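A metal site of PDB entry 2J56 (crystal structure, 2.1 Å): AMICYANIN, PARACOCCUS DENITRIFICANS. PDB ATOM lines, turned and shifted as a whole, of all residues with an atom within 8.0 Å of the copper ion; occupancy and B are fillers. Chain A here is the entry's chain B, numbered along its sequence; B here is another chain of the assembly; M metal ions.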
ATOM      1  N   ILE A  25     -29.172 -10.063  -0.970  1.00  0.00           N
ATOM      2  CA  ILE A  25     -28.122  -9.218  -1.519  1.00  0.00           C
ATOM      3  C   ILE A  25     -27.419 -10.050  -2.574  1.00  0.00           C
ATOM      4  O   ILE A  25     -26.941 -11.140  -2.293  1.00  0.00           O
ATOM      5  CB  ILE A  25     -27.090  -8.829  -0.448  1.00  0.00           C
ATOM      6  CG1 ILE A  25     -27.786  -8.308   0.836  1.00  0.00           C
ATOM      7  CG2 ILE A  25     -26.065  -7.805  -1.036  1.00  0.00           C
ATOM      8  CD1 ILE A  25     -26.771  -7.981   2.005  1.00  0.00           C
ATOM      9  N   MET A  28     -24.206  -7.303  -6.401  1.00  0.00           N
ATOM     10  CA  MET A  28     -23.792  -5.974  -5.967  1.00  0.00           C
ATOM     11  C   MET A  28     -24.961  -5.041  -5.718  1.00  0.00           C
ATOM     12  O   MET A  28     -24.809  -3.840  -5.877  1.00  0.00           O
ATOM     13  CB  MET A  28     -22.797  -5.345  -6.984  1.00  0.00           C
ATOM     14  CG  MET A  28     -21.561  -6.221  -7.263  1.00  0.00           C
ATOM     15  SD  MET A  28     -20.624  -6.644  -5.755  1.00  0.00           S
ATOM     16  CE  MET A  28     -20.090  -4.971  -5.295  1.00  0.00           C
ATOM     17  N   LYS A  29     -26.124  -5.594  -5.304  1.00  0.00           N
ATOM     18  CA  LYS A  29     -27.326  -4.804  -5.089  1.00  0.00           C
ATOM     19  C   LYS A  29     -28.100  -5.368  -3.920  1.00  0.00           C
ATOM     20  O   LYS A  29     -28.140  -6.592  -3.751  1.00  0.00           O
ATOM     21  CB  LYS A  29     -28.272  -4.934  -6.313  1.00  0.00           C
ATOM     22  CG  LYS A  29     -28.060  -3.900  -7.389  1.00  0.00           C
ATOM     23  CD  LYS A  29     -28.722  -4.271  -8.770  1.00  0.00           C
ATOM     24  CE  LYS A  29     -28.320  -3.167  -9.804  1.00  0.00           C
ATOM     25  NZ  LYS A  29     -28.540  -3.357 -11.303  1.00  0.00           N
ATOM     26  N   TYR A  30     -28.721  -4.490  -3.148  1.00  0.00           N
ATOM     27  CA  TYR A  30     -29.760  -4.927  -2.238  1.00  0.00           C
ATOM     28  C   TYR A  30     -31.018  -5.191  -3.095  1.00  0.00           C
ATOM     29  O   TYR A  30     -31.199  -4.542  -4.120  1.00  0.00           O
ATOM     30  CB  TYR A  30     -30.063  -3.839  -1.178  1.00  0.00           C
ATOM     31  CG  TYR A  30     -28.882  -3.463  -0.279  1.00  0.00           C
ATOM     32  CD1 TYR A  30     -28.328  -4.396   0.594  1.00  0.00           C
ATOM     33  CD2 TYR A  30     -28.348  -2.168  -0.296  1.00  0.00           C
ATOM     34  CE1 TYR A  30     -27.236  -4.037   1.463  1.00  0.00           C
ATOM     35  CE2 TYR A  30     -27.287  -1.792   0.526  1.00  0.00           C
ATOM     36  CZ  TYR A  30     -26.736  -2.738   1.404  1.00  0.00           C
ATOM     37  OH  TYR A  30     -25.692  -2.357   2.209  1.00  0.00           O
ATOM     38  N   ASN A  47     -26.843 -12.295   2.416  1.00  0.00           N
ATOM     39  CA  ASN A  47     -25.938 -12.168   1.290  1.00  0.00           C
ATOM     40  C   ASN A  47     -25.958 -13.490   0.499  1.00  0.00           C
ATOM     41  O   ASN A  47     -25.666 -14.562   1.045  1.00  0.00           O
ATOM     42  CB  ASN A  47     -24.505 -11.821   1.769  1.00  0.00           C
ATOM     43  CG  ASN A  47     -23.566 -11.619   0.633  1.00  0.00           C
ATOM     44  OD1 ASN A  47     -24.006 -11.570  -0.527  1.00  0.00           O
ATOM     45  ND2 ASN A  47     -22.248 -11.530   0.930  1.00  0.00           N
ATOM     46  N   GLU A  49     -24.147 -14.019  -2.340  1.00  0.00           N
ATOM     47  CA  GLU A  49     -22.972 -14.137  -3.202  1.00  0.00           C
ATOM     48  C   GLU A  49     -21.652 -14.101  -2.422  1.00  0.00           C
ATOM     49  O   GLU A  49     -21.631 -13.769  -1.235  1.00  0.00           O
ATOM     50  CB  GLU A  49     -23.007 -13.060  -4.297  1.00  0.00           C
ATOM     51  CG  GLU A  49     -23.029 -11.575  -3.792  1.00  0.00           C
ATOM     52  CD  GLU A  49     -22.806 -10.551  -4.918  1.00  0.00           C
ATOM     53  OE1 GLU A  49     -22.425 -10.968  -6.026  1.00  0.00           O
ATOM     54  OE2 GLU A  49     -22.991  -9.330  -4.702  1.00  0.00           O
ATOM     55  N   MET A  51     -18.836 -12.216  -2.734  1.00  0.00           N
ATOM     56  CA  MET A  51     -18.502 -10.833  -2.364  1.00  0.00           C
ATOM     57  C   MET A  51     -19.102 -10.440  -0.997  1.00  0.00           C
ATOM     58  O   MET A  51     -20.323 -10.509  -0.810  1.00  0.00           O
ATOM     59  CB  MET A  51     -19.014  -9.861  -3.420  1.00  0.00           C
ATOM     60  CG  MET A  51     -18.713  -8.383  -3.105  1.00  0.00           C
ATOM     61  SD  MET A  51     -16.920  -7.993  -3.211  1.00  0.00           S
ATOM     62  CE  MET A  51     -16.738  -7.925  -4.990  1.00  0.00           C
ATOM     63  N   PRO A  52     -18.253 -10.107  -0.020  1.00  0.00           N
ATOM     64  CA  PRO A  52     -18.818  -9.730   1.281  1.00  0.00           C
ATOM     65  C   PRO A  52     -19.571  -8.396   1.237  1.00  0.00           C
ATOM     66  O   PRO A  52     -19.143  -7.433   0.565  1.00  0.00           O
ATOM     67  CB  PRO A  52     -17.578  -9.668   2.193  1.00  0.00           C
ATOM     68  CG  PRO A  52     -16.570 -10.577   1.470  1.00  0.00           C
ATOM     69  CD  PRO A  52     -16.792 -10.171   0.027  1.00  0.00           C
ATOM     70  N   HIS A  53     -20.687  -8.344   1.973  1.00  0.00           N
ATOM     71  CA  HIS A  53     -21.452  -7.105   2.078  1.00  0.00           C
ATOM     72  C   HIS A  53     -21.884  -6.921   3.513  1.00  0.00           C
ATOM     73  O   HIS A  53     -21.964  -7.887   4.259  1.00  0.00           O
ATOM     74  CB  HIS A  53     -22.728  -7.216   1.197  1.00  0.00           C
ATOM     75  CG  HIS A  53     -22.448  -7.429  -0.261  1.00  0.00           C
ATOM     76  ND1 HIS A  53     -21.885  -6.467  -1.069  1.00  0.00           N
ATOM     77  CD2 HIS A  53     -22.688  -8.505  -1.069  1.00  0.00           C
ATOM     78  CE1 HIS A  53     -21.801  -6.918  -2.301  1.00  0.00           C
ATOM     79  NE2 HIS A  53     -22.276  -8.150  -2.341  1.00  0.00           N
ATOM     80  N   ASN A  54     -22.229  -5.694   3.880  1.00  0.00           N
ATOM     81  CA  ASN A  54     -22.942  -5.450   5.144  1.00  0.00           C
ATOM     82  C   ASN A  54     -24.005  -4.405   4.922  1.00  0.00           C
ATOM     83  O   ASN A  54     -24.294  -4.009   3.780  1.00  0.00           O
ATOM     84  CB  ASN A  54     -21.977  -5.018   6.273  1.00  0.00           C
ATOM     85  CG  ASN A  54     -21.409  -3.635   6.069  1.00  0.00           C
ATOM     86  OD1 ASN A  54     -21.450  -3.095   4.953  1.00  0.00           O
ATOM     87  ND2 ASN A  54     -20.893  -3.036   7.147  1.00  0.00           N
ATOM     88  N   VAL A  55     -24.576  -3.950   6.046  1.00  0.00           N
ATOM     89  CA  VAL A  55     -25.429  -2.775   6.089  1.00  0.00           C
ATOM     90  C   VAL A  55     -24.817  -1.817   7.113  1.00  0.00           C
ATOM     91  O   VAL A  55     -24.336  -2.234   8.174  1.00  0.00           O
ATOM     92  CB  VAL A  55     -26.921  -3.111   6.436  1.00  0.00           C
ATOM     93  CG1 VAL A  55     -27.502  -4.009   5.318  1.00  0.00           C
ATOM     94  CG2 VAL A  55     -27.074  -3.814   7.784  1.00  0.00           C
ATOM     95  N   MET A  71     -19.575  -7.680   8.209  1.00  0.00           N
ATOM     96  CA  MET A  71     -19.554  -8.196   6.840  1.00  0.00           C
ATOM     97  C   MET A  71     -20.099  -9.638   6.794  1.00  0.00           C
ATOM     98  O   MET A  71     -19.755 -10.495   7.636  1.00  0.00           O
ATOM     99  CB  MET A  71     -18.142  -8.189   6.250  1.00  0.00           C
ATOM    100  CG  MET A  71     -17.495  -6.812   6.142  1.00  0.00           C
ATOM    101  SD  MET A  71     -18.459  -5.547   5.233  1.00  0.00           S
ATOM    102  CE  MET A  71     -18.200  -6.066   3.541  1.00  0.00           C
ATOM    103  N   MET A  72     -20.970  -9.879   5.833  1.00  0.00           N
ATOM    104  CA  MET A  72     -21.546 -11.179   5.629  1.00  0.00           C
ATOM    105  C   MET A  72     -20.806 -11.850   4.475  1.00  0.00           C
ATOM    106  O   MET A  72     -20.587 -11.269   3.429  1.00  0.00           O
ATOM    107  CB  MET A  72     -23.037 -11.061   5.309  1.00  0.00           C
ATOM    108  CG  MET A  72     -23.894 -10.566   6.454  1.00  0.00           C
ATOM    109  SD  MET A  72     -25.584 -10.220   5.868  1.00  0.00           S
ATOM    110  CE  MET A  72     -25.348  -8.532   5.324  1.00  0.00           C
ATOM    111  N   HIS A  91     -26.043   1.887   3.786  1.00  0.00           N
ATOM    112  CA  HIS A  91     -25.158   1.575   2.654  1.00  0.00           C
ATOM    113  C   HIS A  91     -24.253   0.405   3.039  1.00  0.00           C
ATOM    114  O   HIS A  91     -24.274  -0.062   4.209  1.00  0.00           O
ATOM    115  CB  HIS A  91     -24.336   2.775   2.179  1.00  0.00           C
ATOM    116  CG  HIS A  91     -23.191   3.153   3.082  1.00  0.00           C
ATOM    117  ND1 HIS A  91     -23.336   3.967   4.186  1.00  0.00           N
ATOM    118  CD2 HIS A  91     -21.861   2.870   3.004  1.00  0.00           C
ATOM    119  CE1 HIS A  91     -22.167   4.152   4.760  1.00  0.00           C
ATOM    120  NE2 HIS A  91     -21.253   3.507   4.056  1.00  0.00           N
ATOM    121  N   CYS A  92     -23.503  -0.090   2.058  1.00  0.00           N
ATOM    122  CA  CYS A  92     -22.579  -1.177   2.289  1.00  0.00           C
ATOM    123  C   CYS A  92     -21.177  -0.585   2.421  1.00  0.00           C
ATOM    124  O   CYS A  92     -20.685   0.132   1.534  1.00  0.00           O
ATOM    125  CB  CYS A  92     -22.638  -2.217   1.176  1.00  0.00           C
ATOM    126  SG  CYS A  92     -21.410  -3.486   1.382  1.00  0.00           S
ATOM    127  N   THR A  93     -20.545  -0.846   3.553  1.00  0.00           N
ATOM    128  CA  THR A  93     -19.329  -0.055   3.926  1.00  0.00           C
ATOM    129  C   THR A  93     -18.288   0.122   2.808  1.00  0.00           C
ATOM    130  O   THR A  93     -17.925   1.244   2.521  1.00  0.00           O
ATOM    131  CB  THR A  93     -18.684  -0.544   5.211  1.00  0.00           C
ATOM    132  OG1 THR A  93     -19.648  -0.519   6.272  1.00  0.00           O
ATOM    133  CG2 THR A  93     -17.484   0.316   5.602  1.00  0.00           C
ATOM    134  N   PRO A  94     -17.808  -0.971   2.168  1.00  0.00           N
ATOM    135  CA  PRO A  94     -16.862  -0.774   1.059  1.00  0.00           C
ATOM    136  C   PRO A  94     -17.508  -0.367  -0.264  1.00  0.00           C
ATOM    137  O   PRO A  94     -16.761  -0.045  -1.211  1.00  0.00           O
ATOM    138  CB  PRO A  94     -16.310  -2.168   0.871  1.00  0.00           C
ATOM    139  CG  PRO A  94     -17.435  -3.044   1.196  1.00  0.00           C
ATOM    140  CD  PRO A  94     -18.038  -2.406   2.401  1.00  0.00           C
ATOM    141  N   HIS A  95     -18.839  -0.465  -0.365  1.00  0.00           N
ATOM    142  CA  HIS A  95     -19.536  -0.228  -1.633  1.00  0.00           C
ATOM    143  C   HIS A  95     -20.628   0.807  -1.467  1.00  0.00           C
ATOM    144  O   HIS A  95     -21.822   0.481  -1.404  1.00  0.00           O
ATOM    145  CB  HIS A  95     -20.183  -1.486  -2.190  1.00  0.00           C
ATOM    146  CG  HIS A  95     -19.305  -2.696  -2.142  1.00  0.00           C
ATOM    147  ND1 HIS A  95     -19.799  -3.927  -1.765  1.00  0.00           N
ATOM    148  CD2 HIS A  95     -17.988  -2.871  -2.404  1.00  0.00           C
ATOM    149  CE1 HIS A  95     -18.811  -4.801  -1.780  1.00  0.00           C
ATOM    150  NE2 HIS A  95     -17.706  -4.189  -2.166  1.00  0.00           N
ATOM    151  N   PRO A  96     -20.237   2.087  -1.387  1.00  0.00           N
ATOM    152  CA  PRO A  96     -21.170   3.178  -1.121  1.00  0.00           C
ATOM    153  C   PRO A  96     -22.236   3.310  -2.194  1.00  0.00           C
ATOM    154  O   PRO A  96     -23.259   3.960  -1.943  1.00  0.00           O
ATOM    155  CB  PRO A  96     -20.268   4.423  -1.139  1.00  0.00           C
ATOM    156  CG  PRO A  96     -18.905   3.916  -0.926  1.00  0.00           C
ATOM    157  CD  PRO A  96     -18.861   2.554  -1.549  1.00  0.00           C
ATOM    158  N   PHE A  97     -21.976   2.728  -3.374  1.00  0.00           N
ATOM    159  CA  PHE A  97     -22.966   2.626  -4.461  1.00  0.00           C
ATOM    160  C   PHE A  97     -24.100   1.637  -4.193  1.00  0.00           C
ATOM    161  O   PHE A  97     -25.074   1.589  -4.952  1.00  0.00           O
ATOM    162  CB  PHE A  97     -22.270   2.264  -5.781  1.00  0.00           C
ATOM    163  CG  PHE A  97     -21.451   1.006  -5.696  1.00  0.00           C
ATOM    164  CD1 PHE A  97     -22.040  -0.229  -5.936  1.00  0.00           C
ATOM    165  CD2 PHE A  97     -20.095   1.073  -5.325  1.00  0.00           C
ATOM    166  CE1 PHE A  97     -21.278  -1.375  -5.829  1.00  0.00           C
ATOM    167  CE2 PHE A  97     -19.338  -0.066  -5.222  1.00  0.00           C
ATOM    168  CZ  PHE A  97     -19.935  -1.306  -5.460  1.00  0.00           C
ATOM    169  N   MET A  98     -23.972   0.816  -3.134  1.00  0.00           N
ATOM    170  CA  MET A  98     -25.067  -0.006  -2.627  1.00  0.00           C
ATOM    171  C   MET A  98     -25.793   0.732  -1.494  1.00  0.00           C
ATOM    172  O   MET A  98     -25.266   0.872  -0.382  1.00  0.00           O
ATOM    173  CB  MET A  98     -24.543  -1.359  -2.135  1.00  0.00           C
ATOM    174  CG  MET A  98     -23.744  -2.149  -3.171  1.00  0.00           C
ATOM    175  SD  MET A  98     -23.243  -3.799  -2.588  1.00  0.00           S
ATOM    176  CE  MET A  98     -24.785  -4.508  -2.023  1.00  0.00           C
ATOM    177  N   GLU B 101     -14.980  -2.324  -5.670  1.00  0.00           N
ATOM    178  CA  GLU B 101     -14.928  -3.617  -5.040  1.00  0.00           C
ATOM    179  C   GLU B 101     -13.698  -4.441  -5.449  1.00  0.00           C
ATOM    180  O   GLU B 101     -13.299  -5.354  -4.716  1.00  0.00           O
ATOM    181  CB  GLU B 101     -16.253  -4.389  -5.259  1.00  0.00           C
ATOM    182  CG  GLU B 101     -16.502  -4.879  -6.712  1.00  0.00           C
ATOM    183  CD  GLU B 101     -17.286  -3.902  -7.579  1.00  0.00           C
ATOM    184  OE1 GLU B 101     -17.222  -2.669  -7.326  1.00  0.00           O
ATOM    185  OE2 GLU B 101     -17.959  -4.377  -8.543  1.00  0.00           O
HETATM  186 CU    CU M   1     -21.388  -4.553  -0.626  1.00  0.00          CU
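The side-chain sulfur (SD) of Met 98 sits close to a ring nitrogen (ND1) of His 53. A ring nitrogen (NE2) of His 53 sits close to the backbone carbonyl oxygen of Met 51 (3.4 Å). OE2 of Glu 49 lies within hydrogen-bond range of NE2 of His 53, at 2.7 Å. The backbone carbonyl oxygen (O) of His 53 lies within hydrogen-bond range of the backbone NH (N) of Met 72, 2.7 Å away. The side-chain sulfur of Met 98 sits close to a ring nitrogen (ND1) of His 95. The backbone NH of Cys 92 lies within hydrogen-bond range of the backbone carbonyl oxygen of Met 98, at 3.2 Å. The side-chain sulfur (SG) of Cys 92 sits close to the backbone NH (N) of Asn 54, at 3.4 Å. The side-chain hydroxyl (OH) of Tyr 30 is in hydrogen-bond range of the backbone NH (N) of Cys 92 (3.2 Å).
Pro 52 touches the copper ion. Within 4 Å of the copper ion: Pro 52, His 53, Cys 92, His 95 and Met 98. The nearest printed residue that does not touch the copper ion is Pro 94 (4.6 Å).
The copper ion is bound by ND1 of His 53 (2.0 Å), ND1 of His 95 (2.1 Å) and SG of Cys 92 (2.3 Å). Slightly farther from the copper ion lies the side-chain sulfur (SD) of Met 98 (2.8 Å).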
